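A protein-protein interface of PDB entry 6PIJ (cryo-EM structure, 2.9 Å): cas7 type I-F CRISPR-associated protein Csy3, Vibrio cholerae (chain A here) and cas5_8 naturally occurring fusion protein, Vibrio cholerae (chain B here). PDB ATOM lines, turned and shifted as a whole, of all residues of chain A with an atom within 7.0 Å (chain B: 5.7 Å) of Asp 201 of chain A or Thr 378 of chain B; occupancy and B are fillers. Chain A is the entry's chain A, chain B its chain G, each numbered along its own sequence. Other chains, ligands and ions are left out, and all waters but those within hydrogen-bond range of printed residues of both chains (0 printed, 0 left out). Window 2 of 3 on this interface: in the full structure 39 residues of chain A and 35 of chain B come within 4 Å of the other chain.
OD1 of Asp 201 of chain A is in salt-bridge range of NH1 of Arg 308 of chain B, 3.3 Å away.
OG of Ser 93 of chain A is in hydrogen-bond range of O of Gly 202 of chain A, 3.1 Å away. The guanidinium group (NE) of Arg 308 of chain B is in hydrogen-bond range of the backbone carbonyl oxygen (O) of Asn 305 of chain B. The backbone carbonyl oxygen of Asp 374 of chain B is in hydrogen-bond range of the side-chain hydroxyl of Thr 378 of chain B, 2.7 Å away.
Among the printed residues, merely in contact across the chains: Ser 93 of chain A with Lys 382 of chain B (3.3 Å), Trp 158 of chain A with Val 377 of chain B (3.5 Å), Asp 201 of chain A with Thr 378 of chain B (3.2 Å), Leu 203 of chain A with Val 377 of chain B (3.98 Å), Leu 203 of chain A with Thr 378 of chain B (3.7 Å) and Leu 203 of chain A with Lys 382 of chain B (3.2 Å).
Of the printed residues of chain B, Ser 93 of chain A touches Lys 382. Of chain B, only Arg 308 (3.3 Å) and Thr 378 (3.2 Å) come within 4 Å of Asp 201 of chain A. Gly 202 of chain A touches none of the printed residues of chain B. Of the printed residues of chain A, Arg 308 of chain B touches Asp 201 (3.3 Å). Of the printed residues of chain A, Val 377 of chain B touches Trp 158 and Leu 203. Of chain A, only Asp 201 and Leu 203 come within 4 Å of Thr 378 of chain B. Of the printed residues of chain A, Lys 382 of chain B touches Ser 93 and Leu 203. The nearest residue of chain A that does not touch Thr 378 of chain B is Trp 158 of chain A (4.5 Å).
Of the 11 printed residues of chain A, 4 touch a printed residue of chain B. Printed residues of chain A that touch a printed residue of chain B: Ser 93, Trp 158, Asp 201 and Leu 203. Hydrophobic or aromatic side chains of chain A that line the printed part of chain B: Trp 158 and Leu 203. Hydrophobic or aromatic side chains of chain B within 4 Å of the printed part of chain A: Val 377. Among the printed residues, Asp or Glu carboxylates within 4 Å of a Lys or Arg side-chain nitrogen of the other chain: Asp 201 of chain A with Arg 308 of chain B (3.3 Å).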
ATOM      1  N   SER A  93      -0.371  31.413 -11.093  1.00  0.00           N
ATOM      2  CA  SER A  93      -0.134  31.371  -9.623  1.00  0.00           C
ATOM      3  C   SER A  93       0.442  32.707  -9.132  1.00  0.00           C
ATOM      4  O   SER A  93       0.538  33.644  -9.945  1.00  0.00           O
ATOM      5  CB  SER A  93       0.754  30.206  -9.260  1.00  0.00           C
ATOM      6  OG  SER A  93       1.259  30.318  -7.937  1.00  0.00           O
ATOM      7  N   SER A  94       0.790  32.780  -7.842  1.00  0.00           N
ATOM      8  CA  SER A  94       1.287  33.991  -7.137  1.00  0.00           C
ATOM      9  C   SER A  94       2.695  33.738  -6.581  1.00  0.00           C
ATOM     10  O   SER A  94       2.825  33.539  -5.354  1.00  0.00           O
ATOM     11  CB  SER A  94       0.322  34.397  -6.053  1.00  0.00           C
ATOM     12  OG  SER A  94       0.018  33.300  -5.203  1.00  0.00           O
ATOM     13  N   ARG A  97       4.542  37.456  -5.307  1.00  0.00           N
ATOM     14  CA  ARG A  97       4.312  37.922  -3.910  1.00  0.00           C
ATOM     15  C   ARG A  97       5.608  37.870  -3.087  1.00  0.00           C
ATOM     16  O   ARG A  97       5.681  38.621  -2.097  1.00  0.00           O
ATOM     17  CB  ARG A  97       3.217  37.094  -3.234  1.00  0.00           C
ATOM     18  CG  ARG A  97       1.869  37.190  -3.933  1.00  0.00           C
ATOM     19  CD  ARG A  97       0.690  36.924  -3.017  1.00  0.00           C
ATOM     20  NE  ARG A  97       0.266  38.132  -2.316  1.00  0.00           N
ATOM     21  CZ  ARG A  97      -0.394  39.156  -2.862  1.00  0.00           C
ATOM     22  NH1 ARG A  97      -0.731  39.149  -4.144  1.00  0.00           N
ATOM     23  NH2 ARG A  97      -0.721  40.196  -2.111  1.00  0.00           N
ATOM     24  N   TRP A 158     -10.099  25.771 -13.887  1.00  0.00           N
ATOM     25  CA  TRP A 158      -9.990  25.052 -12.587  1.00  0.00           C
ATOM     26  C   TRP A 158      -9.406  25.986 -11.526  1.00  0.00           C
ATOM     27  O   TRP A 158      -8.392  26.631 -11.788  1.00  0.00           O
ATOM     28  CB  TRP A 158      -9.140  23.788 -12.756  1.00  0.00           C
ATOM     29  CG  TRP A 158      -9.238  22.817 -11.621  1.00  0.00           C
ATOM     30  CD1 TRP A 158     -10.014  21.696 -11.564  1.00  0.00           C
ATOM     31  CD2 TRP A 158      -8.525  22.875 -10.371  1.00  0.00           C
ATOM     32  NE1 TRP A 158      -9.836  21.052 -10.369  1.00  0.00           N
ATOM     33  CE2 TRP A 158      -8.930  21.752  -9.616  1.00  0.00           C
ATOM     34  CE3 TRP A 158      -7.590  23.758  -9.817  1.00  0.00           C
ATOM     35  CZ2 TRP A 158      -8.431  21.495  -8.339  1.00  0.00           C
ATOM     36  CZ3 TRP A 158      -7.098  23.506  -8.554  1.00  0.00           C
ATOM     37  CH2 TRP A 158      -7.514  22.388  -7.827  1.00  0.00           C
ATOM     38  N   THR A 195      -7.934  36.318  -8.263  1.00  0.00           N
ATOM     39  CA  THR A 195      -7.839  35.425  -7.074  1.00  0.00           C
ATOM     40  C   THR A 195      -6.440  34.797  -7.017  1.00  0.00           C
ATOM     41  O   THR A 195      -5.796  34.904  -5.953  1.00  0.00           O
ATOM     42  CB  THR A 195      -8.927  34.341  -7.099  1.00  0.00           C
ATOM     43  OG1 THR A 195     -10.194  34.989  -6.977  1.00  0.00           O
ATOM     44  CG2 THR A 195      -8.777  33.308  -6.002  1.00  0.00           C
ATOM     45  N   ALA A 196      -6.002  34.178  -8.121  1.00  0.00           N
ATOM     46  CA  ALA A 196      -4.707  33.464  -8.249  1.00  0.00           C
ATOM     47  C   ALA A 196      -3.544  34.402  -7.903  1.00  0.00           C
ATOM     48  O   ALA A 196      -2.659  33.966  -7.147  1.00  0.00           O
ATOM     49  CB  ALA A 196      -4.550  32.885  -9.635  1.00  0.00           C
ATOM     50  N   SER A 199      -4.290  36.106  -3.919  1.00  0.00           N
ATOM     51  CA  SER A 199      -4.196  35.097  -2.827  1.00  0.00           C
ATOM     52  C   SER A 199      -2.787  34.494  -2.772  1.00  0.00           C
ATOM     53  O   SER A 199      -2.125  34.429  -3.828  1.00  0.00           O
ATOM     54  CB  SER A 199      -5.236  34.017  -2.990  1.00  0.00           C
ATOM     55  OG  SER A 199      -5.236  33.138  -1.874  1.00  0.00           O
ATOM     56  N   THR A 200      -2.357  34.071  -1.576  1.00  0.00           N
ATOM     57  CA  THR A 200      -1.157  33.219  -1.341  1.00  0.00           C
ATOM     58  C   THR A 200      -1.542  31.756  -1.579  1.00  0.00           C
ATOM     59  O   THR A 200      -2.670  31.379  -1.197  1.00  0.00           O
ATOM     60  CB  THR A 200      -0.590  33.404   0.073  1.00  0.00           C
ATOM     61  OG1 THR A 200      -1.630  33.140   1.015  1.00  0.00           O
ATOM     62  CG2 THR A 200      -0.029  34.788   0.308  1.00  0.00           C
ATOM     63  N   ASP A 201      -0.633  30.972  -2.172  1.00  0.00           N
ATOM     64  CA  ASP A 201      -0.885  29.584  -2.652  1.00  0.00           C
ATOM     65  C   ASP A 201      -2.062  29.611  -3.639  1.00  0.00           C
ATOM     66  O   ASP A 201      -2.930  28.719  -3.556  1.00  0.00           O
ATOM     67  CB  ASP A 201      -1.119  28.623  -1.481  1.00  0.00           C
ATOM     68  CG  ASP A 201      -0.027  28.642  -0.422  1.00  0.00           C
ATOM     69  OD1 ASP A 201       1.069  29.168  -0.711  1.00  0.00           O
ATOM     70  OD2 ASP A 201      -0.281  28.128   0.685  1.00  0.00           O
ATOM     71  N   GLY A 202      -2.091  30.615  -4.525  1.00  0.00           N
ATOM     72  CA  GLY A 202      -3.118  30.777  -5.571  1.00  0.00           C
ATOM     73  C   GLY A 202      -2.815  29.896  -6.769  1.00  0.00           C
ATOM     74  O   GLY A 202      -1.618  29.700  -7.068  1.00  0.00           O
ATOM     75  N   LEU A 203      -3.857  29.375  -7.423  1.00  0.00           N
ATOM     76  CA  LEU A 203      -3.744  28.487  -8.611  1.00  0.00           C
ATOM     77  C   LEU A 203      -4.996  28.641  -9.481  1.00  0.00           C
ATOM     78  O   LEU A 203      -6.105  28.413  -8.959  1.00  0.00           O
ATOM     79  CB  LEU A 203      -3.571  27.039  -8.138  1.00  0.00           C
ATOM     80  CG  LEU A 203      -3.431  25.985  -9.240  1.00  0.00           C
ATOM     81  CD1 LEU A 203      -2.151  26.190 -10.031  1.00  0.00           C
ATOM     82  CD2 LEU A 203      -3.464  24.580  -8.662  1.00  0.00           C
ATOM     83  N   ASN B 305       5.864  21.854   0.125  1.00  0.00           N
ATOM     84  CA  ASN B 305       4.615  22.561  -0.276  1.00  0.00           C
ATOM     85  C   ASN B 305       3.410  22.036   0.525  1.00  0.00           C
ATOM     86  O   ASN B 305       2.433  22.802   0.642  1.00  0.00           O
ATOM     87  CB  ASN B 305       4.362  22.483  -1.787  1.00  0.00           C
ATOM     88  CG  ASN B 305       5.210  23.442  -2.599  1.00  0.00           C
ATOM     89  OD1 ASN B 305       6.105  24.102  -2.073  1.00  0.00           O
ATOM     90  ND2 ASN B 305       4.936  23.525  -3.890  1.00  0.00           N
ATOM     91  N   ARG B 308       3.653  23.122   4.898  1.00  0.00           N
ATOM     92  CA  ARG B 308       3.123  24.461   5.290  1.00  0.00           C
ATOM     93  C   ARG B 308       1.654  24.371   5.745  1.00  0.00           C
ATOM     94  O   ARG B 308       1.157  25.386   6.276  1.00  0.00           O
ATOM     95  CB  ARG B 308       3.304  25.471   4.150  1.00  0.00           C
ATOM     96  CG  ARG B 308       2.450  25.217   2.914  1.00  0.00           C
ATOM     97  CD  ARG B 308       3.012  25.918   1.689  1.00  0.00           C
ATOM     98  NE  ARG B 308       2.297  25.594   0.458  1.00  0.00           N
ATOM     99  CZ  ARG B 308       2.550  26.121  -0.742  1.00  0.00           C
ATOM    100  NH1 ARG B 308       3.512  27.018  -0.901  1.00  0.00           N
ATOM    101  NH2 ARG B 308       1.831  25.746  -1.788  1.00  0.00           N
ATOM    102  N   GLN B 373      -7.693  17.151  -1.472  1.00  0.00           N
ATOM    103  CA  GLN B 373      -7.540  17.275  -2.951  1.00  0.00           C
ATOM    104  C   GLN B 373      -7.241  18.733  -3.335  1.00  0.00           C
ATOM    105  O   GLN B 373      -6.376  18.930  -4.213  1.00  0.00           O
ATOM    106  CB  GLN B 373      -8.784  16.746  -3.667  1.00  0.00           C
ATOM    107  CG  GLN B 373      -8.687  16.823  -5.187  1.00  0.00           C
ATOM    108  CD  GLN B 373      -9.658  15.922  -5.913  1.00  0.00           C
ATOM    109  OE1 GLN B 373     -10.557  15.327  -5.322  1.00  0.00           O
ATOM    110  NE2 GLN B 373      -9.484  15.821  -7.220  1.00  0.00           N
ATOM    111  N   ASP B 374      -7.935  19.708  -2.728  1.00  0.00           N
ATOM    112  CA  ASP B 374      -7.724  21.167  -2.950  1.00  0.00           C
ATOM    113  C   ASP B 374      -6.270  21.529  -2.620  1.00  0.00           C
ATOM    114  O   ASP B 374      -5.631  22.204  -3.451  1.00  0.00           O
ATOM    115  CB  ASP B 374      -8.696  22.018  -2.125  1.00  0.00           C
ATOM    116  CG  ASP B 374     -10.151  21.927  -2.559  1.00  0.00           C
ATOM    117  OD1 ASP B 374     -10.399  21.735  -3.768  1.00  0.00           O
ATOM    118  OD2 ASP B 374     -11.030  22.053  -1.682  1.00  0.00           O
ATOM    119  N   THR B 375      -5.776  21.094  -1.455  1.00  0.00           N
ATOM    120  CA  THR B 375      -4.362  21.254  -1.012  1.00  0.00           C
ATOM    121  C   THR B 375      -3.445  20.408  -1.906  1.00  0.00           C
ATOM    122  O   THR B 375      -2.418  20.945  -2.352  1.00  0.00           O
ATOM    123  CB  THR B 375      -4.188  20.884   0.469  1.00  0.00           C
ATOM    124  OG1 THR B 375      -4.957  21.805   1.244  1.00  0.00           O
ATOM    125  CG2 THR B 375      -2.746  20.912   0.933  1.00  0.00           C
ATOM    126  N   LEU B 376      -3.816  19.148  -2.159  1.00  0.00           N
ATOM    127  CA  LEU B 376      -2.939  18.118  -2.787  1.00  0.00           C
ATOM    128  C   LEU B 376      -2.643  18.463  -4.255  1.00  0.00           C
ATOM    129  O   LEU B 376      -1.584  18.023  -4.746  1.00  0.00           O
ATOM    130  CB  LEU B 376      -3.596  16.738  -2.657  1.00  0.00           C
ATOM    131  CG  LEU B 376      -2.643  15.545  -2.730  1.00  0.00           C
ATOM    132  CD1 LEU B 376      -1.669  15.556  -1.559  1.00  0.00           C
ATOM    133  CD2 LEU B 376      -3.417  14.237  -2.764  1.00  0.00           C
ATOM    134  N   VAL B 377      -3.530  19.211  -4.926  1.00  0.00           N
ATOM    135  CA  VAL B 377      -3.322  19.719  -6.319  1.00  0.00           C
ATOM    136  C   VAL B 377      -2.507  21.018  -6.261  1.00  0.00           C
ATOM    137  O   VAL B 377      -1.502  21.106  -6.988  1.00  0.00           O
ATOM    138  CB  VAL B 377      -4.658  19.915  -7.066  1.00  0.00           C
ATOM    139  CG1 VAL B 377      -4.500  20.753  -8.331  1.00  0.00           C
ATOM    140  CG2 VAL B 377      -5.309  18.580  -7.394  1.00  0.00           C
ATOM    141  N   THR B 378      -2.934  21.989  -5.443  1.00  0.00           N
ATOM    142  CA  THR B 378      -2.344  23.355  -5.357  1.00  0.00           C
ATOM    143  C   THR B 378      -0.906  23.292  -4.827  1.00  0.00           C
ATOM    144  O   THR B 378      -0.102  24.159  -5.227  1.00  0.00           O
ATOM    145  CB  THR B 378      -3.203  24.292  -4.499  1.00  0.00           C
ATOM    146  OG1 THR B 378      -4.562  24.173  -4.920  1.00  0.00           O
ATOM    147  CG2 THR B 378      -2.772  25.739  -4.599  1.00  0.00           C
ATOM    148  N   SER B 379      -0.593  22.306  -3.978  1.00  0.00           N
ATOM    149  CA  SER B 379       0.755  22.062  -3.400  1.00  0.00           C
ATOM    150  C   SER B 379       1.545  21.086  -4.285  1.00  0.00           C
ATOM    151  O   SER B 379       2.191  20.179  -3.721  1.00  0.00           O
ATOM    152  CB  SER B 379       0.643  21.565  -1.976  1.00  0.00           C
ATOM    153  OG  SER B 379       0.071  20.265  -1.933  1.00  0.00           O
ATOM    154  N   LEU B 380       1.502  21.267  -5.613  1.00  0.00           N
ATOM    155  CA  LEU B 380       2.320  20.503  -6.597  1.00  0.00           C
ATOM    156  C   LEU B 380       3.447  21.398  -7.104  1.00  0.00           C
ATOM    157  O   LEU B 380       3.220  22.572  -7.397  1.00  0.00           O
ATOM    158  CB  LEU B 380       1.455  20.015  -7.767  1.00  0.00           C
ATOM    159  CG  LEU B 380       0.904  18.592  -7.656  1.00  0.00           C
ATOM    160  CD1 LEU B 380      -0.023  18.283  -8.822  1.00  0.00           C
ATOM    161  CD2 LEU B 380       2.030  17.566  -7.599  1.00  0.00           C
ATOM    162  N   LYS B 382       5.680  22.876  -9.953  1.00  0.00           N
ATOM    163  CA  LYS B 382       5.265  23.213 -11.342  1.00  0.00           C
ATOM    164  C   LYS B 382       6.439  23.070 -12.320  1.00  0.00           C
ATOM    165  O   LYS B 382       6.322  23.593 -13.448  1.00  0.00           O
ATOM    166  CB  LYS B 382       4.716  24.641 -11.374  1.00  0.00           C
ATOM    167  CG  LYS B 382       3.482  24.867 -10.518  1.00  0.00           C
ATOM    168  CD  LYS B 382       2.854  26.212 -10.767  1.00  0.00           C
ATOM    169  CE  LYS B 382       1.447  26.332 -10.231  1.00  0.00           C
ATOM    170  NZ  LYS B 382       0.719  27.411 -10.936  1.00  0.00           N
